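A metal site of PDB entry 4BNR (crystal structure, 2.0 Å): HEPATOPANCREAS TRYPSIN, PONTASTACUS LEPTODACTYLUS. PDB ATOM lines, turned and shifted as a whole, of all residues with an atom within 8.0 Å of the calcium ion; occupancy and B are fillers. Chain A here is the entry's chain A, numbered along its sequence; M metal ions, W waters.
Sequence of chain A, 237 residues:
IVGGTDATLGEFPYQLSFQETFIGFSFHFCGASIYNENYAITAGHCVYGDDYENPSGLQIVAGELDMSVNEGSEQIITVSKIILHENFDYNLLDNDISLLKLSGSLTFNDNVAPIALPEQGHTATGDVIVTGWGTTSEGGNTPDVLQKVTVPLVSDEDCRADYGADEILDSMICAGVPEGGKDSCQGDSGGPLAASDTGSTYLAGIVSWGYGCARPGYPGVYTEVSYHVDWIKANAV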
ATOM      1  N   LEU A   9      -4.959 -28.543 -25.921  1.00  0.00           N
ATOM      2  CA  LEU A   9      -4.544 -28.038 -24.621  1.00  0.00           C
ATOM      3  C   LEU A   9      -3.020 -27.925 -24.580  1.00  0.00           C
ATOM      4  O   LEU A   9      -2.307 -28.876 -24.881  1.00  0.00           O
ATOM      5  CB  LEU A   9      -5.055 -28.963 -23.520  1.00  0.00           C
ATOM      6  CG  LEU A   9      -4.892 -28.524 -22.067  1.00  0.00           C
ATOM      7  CD1 LEU A   9      -5.617 -27.205 -21.790  1.00  0.00           C
ATOM      8  CD2 LEU A   9      -5.383 -29.630 -21.141  1.00  0.00           C
ATOM      9  N   VAL A  61      -9.456 -16.299 -17.379  1.00  0.00           N
ATOM     10  CA  VAL A  61      -9.286 -17.733 -17.245  1.00  0.00           C
ATOM     11  C   VAL A  61      -8.108 -18.154 -18.092  1.00  0.00           C
ATOM     12  O   VAL A  61      -8.109 -17.948 -19.309  1.00  0.00           O
ATOM     13  CB  VAL A  61     -10.561 -18.511 -17.667  1.00  0.00           C
ATOM     14  CG1 VAL A  61     -10.410 -20.003 -17.369  1.00  0.00           C
ATOM     15  CG2 VAL A  61     -11.760 -17.941 -16.948  1.00  0.00           C
ATOM     16  N   ALA A  62      -7.084 -18.708 -17.435  1.00  0.00           N
ATOM     17  CA  ALA A  62      -5.923 -19.280 -18.103  1.00  0.00           C
ATOM     18  C   ALA A  62      -6.076 -20.797 -18.143  1.00  0.00           C
ATOM     19  O   ALA A  62      -6.807 -21.364 -17.335  1.00  0.00           O
ATOM     20  CB  ALA A  62      -4.643 -18.909 -17.369  1.00  0.00           C
ATOM     21  N   GLY A  63      -5.396 -21.440 -19.077  1.00  0.00           N
ATOM     22  CA  GLY A  63      -5.449 -22.887 -19.200  1.00  0.00           C
ATOM     23  C   GLY A  63      -6.809 -23.394 -19.633  1.00  0.00           C
ATOM     24  O   GLY A  63      -7.186 -24.512 -19.308  1.00  0.00           O
ATOM     25  N   GLU A  64      -7.537 -22.559 -20.362  1.00  0.00           N
ATOM     26  CA  GLU A  64      -8.840 -22.944 -20.873  1.00  0.00           C
ATOM     27  C   GLU A  64      -8.685 -23.464 -22.307  1.00  0.00           C
ATOM     28  O   GLU A  64      -7.815 -23.009 -23.055  1.00  0.00           O
ATOM     29  CB  GLU A  64      -9.782 -21.747 -20.822  1.00  0.00           C
ATOM     30  CG  GLU A  64     -11.202 -22.001 -21.289  1.00  0.00           C
ATOM     31  CD  GLU A  64     -11.892 -23.073 -20.489  1.00  0.00           C
ATOM     32  OE1 GLU A  64     -11.627 -24.247 -20.758  1.00  0.00           O
ATOM     33  OE2 GLU A  64     -12.696 -22.738 -19.582  1.00  0.00           O
ATOM     34  N   LEU A  65      -9.536 -24.410 -22.689  1.00  0.00           N
ATOM     35  CA  LEU A  65      -9.561 -24.883 -24.065  1.00  0.00           C
ATOM     36  C   LEU A  65     -10.995 -25.092 -24.504  1.00  0.00           C
ATOM     37  O   LEU A  65     -11.481 -24.404 -25.402  1.00  0.00           O
ATOM     38  CB  LEU A  65      -8.771 -26.177 -24.229  1.00  0.00           C
ATOM     39  CG  LEU A  65      -8.726 -26.712 -25.661  1.00  0.00           C
ATOM     40  CD1 LEU A  65      -7.646 -25.989 -26.447  1.00  0.00           C
ATOM     41  CD2 LEU A  65      -8.475 -28.188 -25.651  1.00  0.00           C
ATOM     42  N   ASP A  66     -11.651 -26.047 -23.867  1.00  0.00           N
ATOM     43  CA  ASP A  66     -13.058 -26.353 -24.141  1.00  0.00           C
ATOM     44  C   ASP A  66     -13.910 -25.831 -22.992  1.00  0.00           C
ATOM     45  O   ASP A  66     -13.825 -26.320 -21.871  1.00  0.00           O
ATOM     46  CB  ASP A  66     -13.228 -27.866 -24.286  1.00  0.00           C
ATOM     47  CG  ASP A  66     -14.615 -28.262 -24.763  1.00  0.00           C
ATOM     48  OD1 ASP A  66     -15.603 -27.605 -24.384  1.00  0.00           O
ATOM     49  OD2 ASP A  66     -14.704 -29.243 -25.534  1.00  0.00           O
ATOM     50  N   MET A  67     -14.754 -24.856 -23.276  1.00  0.00           N
ATOM     51  CA  MET A  67     -15.533 -24.222 -22.223  1.00  0.00           C
ATOM     52  C   MET A  67     -16.703 -25.071 -21.730  1.00  0.00           C
ATOM     53  O   MET A  67     -17.357 -24.699 -20.745  1.00  0.00           O
ATOM     54  CB  MET A  67     -16.027 -22.849 -22.679  1.00  0.00           C
ATOM     55  CG  MET A  67     -14.898 -21.847 -22.742  1.00  0.00           C
ATOM     56  SD  MET A  67     -15.548 -20.225 -23.090  1.00  0.00           S
ATOM     57  CE  MET A  67     -14.072 -19.241 -22.990  1.00  0.00           C
ATOM     58  N   SER A  68     -16.952 -26.209 -22.368  1.00  0.00           N
ATOM     59  CA  SER A  68     -18.050 -27.094 -21.957  1.00  0.00           C
ATOM     60  C   SER A  68     -17.624 -28.142 -20.926  1.00  0.00           C
ATOM     61  O   SER A  68     -18.487 -28.797 -20.323  1.00  0.00           O
ATOM     62  CB  SER A  68     -18.677 -27.774 -23.182  1.00  0.00           C
ATOM     63  OG  SER A  68     -17.859 -28.819 -23.689  1.00  0.00           O
ATOM     64  N   VAL A  69     -16.328 -28.321 -20.724  1.00  0.00           N
ATOM     65  CA  VAL A  69     -15.830 -29.390 -19.858  1.00  0.00           C
ATOM     66  C   VAL A  69     -14.724 -28.899 -18.936  1.00  0.00           C
ATOM     67  O   VAL A  69     -13.820 -28.182 -19.364  1.00  0.00           O
ATOM     68  CB  VAL A  69     -15.350 -30.611 -20.703  1.00  0.00           C
ATOM     69  CG1 VAL A  69     -14.517 -30.156 -21.897  1.00  0.00           C
ATOM     70  CG2 VAL A  69     -14.578 -31.611 -19.855  1.00  0.00           C
ATOM     71  N   ASN A  70     -14.804 -29.273 -17.669  1.00  0.00           N
ATOM     72  CA  ASN A  70     -13.746 -28.975 -16.708  1.00  0.00           C
ATOM     73  C   ASN A  70     -12.544 -29.880 -16.979  1.00  0.00           C
ATOM     74  O   ASN A  70     -12.574 -31.071 -16.644  1.00  0.00           O
ATOM     75  CB  ASN A  70     -14.262 -29.153 -15.282  1.00  0.00           C
ATOM     76  CG  ASN A  70     -13.203 -28.827 -14.245  1.00  0.00           C
ATOM     77  OD1 ASN A  70     -12.122 -28.325 -14.555  1.00  0.00           O
ATOM     78  ND2 ASN A  70     -13.519 -29.122 -12.986  1.00  0.00           N
ATOM     79  N   GLU A  71     -11.499 -29.323 -17.581  1.00  0.00           N
ATOM     80  CA  GLU A  71     -10.332 -30.104 -18.022  1.00  0.00           C
ATOM     81  C   GLU A  71      -9.238 -30.161 -16.968  1.00  0.00           C
ATOM     82  O   GLU A  71      -8.248 -30.877 -17.120  1.00  0.00           O
ATOM     83  CB  GLU A  71      -9.775 -29.533 -19.341  1.00  0.00           C
ATOM     84  CG  GLU A  71     -10.718 -29.721 -20.526  1.00  0.00           C
ATOM     85  CD  GLU A  71     -10.609 -28.608 -21.563  1.00  0.00           C
ATOM     86  OE1 GLU A  71     -10.842 -27.428 -21.215  1.00  0.00           O
ATOM     87  OE2 GLU A  71     -10.296 -28.931 -22.728  1.00  0.00           O
ATOM     88  N   GLY A  72      -9.425 -29.412 -15.879  1.00  0.00           N
ATOM     89  CA  GLY A  72      -8.502 -29.428 -14.757  1.00  0.00           C
ATOM     90  C   GLY A  72      -7.403 -28.378 -14.848  1.00  0.00           C
ATOM     91  O   GLY A  72      -6.794 -28.041 -13.841  1.00  0.00           O
ATOM     92  N   SER A  73      -7.165 -27.861 -16.052  1.00  0.00           N
ATOM     93  CA  SER A  73      -6.076 -26.886 -16.280  1.00  0.00           C
ATOM     94  C   SER A  73      -6.477 -25.442 -15.989  1.00  0.00           C
ATOM     95  O   SER A  73      -5.624 -24.552 -15.876  1.00  0.00           O
ATOM     96  CB  SER A  73      -5.609 -26.969 -17.738  1.00  0.00           C
ATOM     97  OG  SER A  73      -4.887 -28.153 -17.983  1.00  0.00           O
ATOM     98  N   GLU A  74      -7.776 -25.207 -15.872  1.00  0.00           N
ATOM     99  CA  GLU A  74      -8.289 -23.845 -15.790  1.00  0.00           C
ATOM    100  C   GLU A  74      -7.843 -23.130 -14.513  1.00  0.00           C
ATOM    101  O   GLU A  74      -7.939 -23.675 -13.414  1.00  0.00           O
ATOM    102  CB  GLU A  74      -9.808 -23.849 -15.882  1.00  0.00           C
ATOM    103  CG  GLU A  74     -10.359 -24.513 -17.152  1.00  0.00           C
ATOM    104  CD  GLU A  74     -10.619 -26.014 -16.990  1.00  0.00           C
ATOM    105  OE1 GLU A  74     -10.108 -26.629 -16.039  1.00  0.00           O
ATOM    106  OE2 GLU A  74     -11.344 -26.573 -17.837  1.00  0.00           O
ATOM    107  N   TRP A 133     -12.040 -17.452 -28.749  1.00  0.00           N
ATOM    108  CA  TRP A 133     -13.351 -18.088 -28.702  1.00  0.00           C
ATOM    109  C   TRP A 133     -14.414 -17.169 -29.301  1.00  0.00           C
ATOM    110  O   TRP A 133     -15.573 -17.181 -28.901  1.00  0.00           O
ATOM    111  CB  TRP A 133     -13.748 -18.426 -27.258  1.00  0.00           C
ATOM    112  CG  TRP A 133     -12.970 -19.548 -26.588  1.00  0.00           C
ATOM    113  CD1 TRP A 133     -13.266 -20.883 -26.603  1.00  0.00           C
ATOM    114  CD2 TRP A 133     -11.789 -19.411 -25.776  1.00  0.00           C
ATOM    115  NE1 TRP A 133     -12.336 -21.583 -25.873  1.00  0.00           N
ATOM    116  CE2 TRP A 133     -11.431 -20.718 -25.351  1.00  0.00           C
ATOM    117  CE3 TRP A 133     -11.008 -18.325 -25.385  1.00  0.00           C
ATOM    118  CZ2 TRP A 133     -10.309 -20.948 -24.544  1.00  0.00           C
ATOM    119  CZ3 TRP A 133      -9.900 -18.560 -24.580  1.00  0.00           C
ATOM    120  CH2 TRP A 133      -9.558 -19.856 -24.174  1.00  0.00           C
ATOM    121  N   ASP A 144     -17.209 -23.846 -28.366  1.00  0.00           N
ATOM    122  CA  ASP A 144     -16.775 -24.290 -27.046  1.00  0.00           C
ATOM    123  C   ASP A 144     -15.266 -24.412 -27.019  1.00  0.00           C
ATOM    124  O   ASP A 144     -14.632 -24.107 -26.002  1.00  0.00           O
ATOM    125  CB  ASP A 144     -17.398 -25.638 -26.690  1.00  0.00           C
ATOM    126  CG  ASP A 144     -18.905 -25.569 -26.505  1.00  0.00           C
ATOM    127  OD1 ASP A 144     -19.414 -24.478 -26.181  1.00  0.00           O
ATOM    128  OD2 ASP A 144     -19.570 -26.610 -26.674  1.00  0.00           O
HETATM  129 CA    CA M   1     -12.516 -26.258 -19.891  1.00  0.00          CA
HETATM  130  O   HOH W   1     -13.959 -25.106 -18.926  1.00  0.00           O
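Within 4 Å of the calcium ion: Glu 64, Asp 66, Val 69, Glu 71 and Glu 74.
The nearest printed residue that does not touch the calcium ion is Met 67 (4.3 Å).
OD1 of Asp 66 sits at hydrogen-bond distance from OG of Ser 68 (2.7 Å).
The side-chain carboxylate of Glu 74 sits close to the side-chain amide oxygen of Asn 70 (3.0 Å).
The side-chain carboxylate of Glu 74 is in hydrogen-bond range of the backbone NH of Gly 72, 2.9 Å away.
Water W1 is bound to the calcium ion (2.1 Å).
The calcium ion is bound by OE1 of Glu 64, 2.4 Å away.
The calcium ion is bound by O of Asp 66.
O of Val 69 is bound to the calcium ion (2.4 Å).
The side-chain carboxylate (OE2) of Glu 74 is bound to the calcium ion, at 2.4 Å.
The calcium ion is bound by OE1 of Glu 71 (2.4 Å).
The calcium ion has six donor atoms within binding distance.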
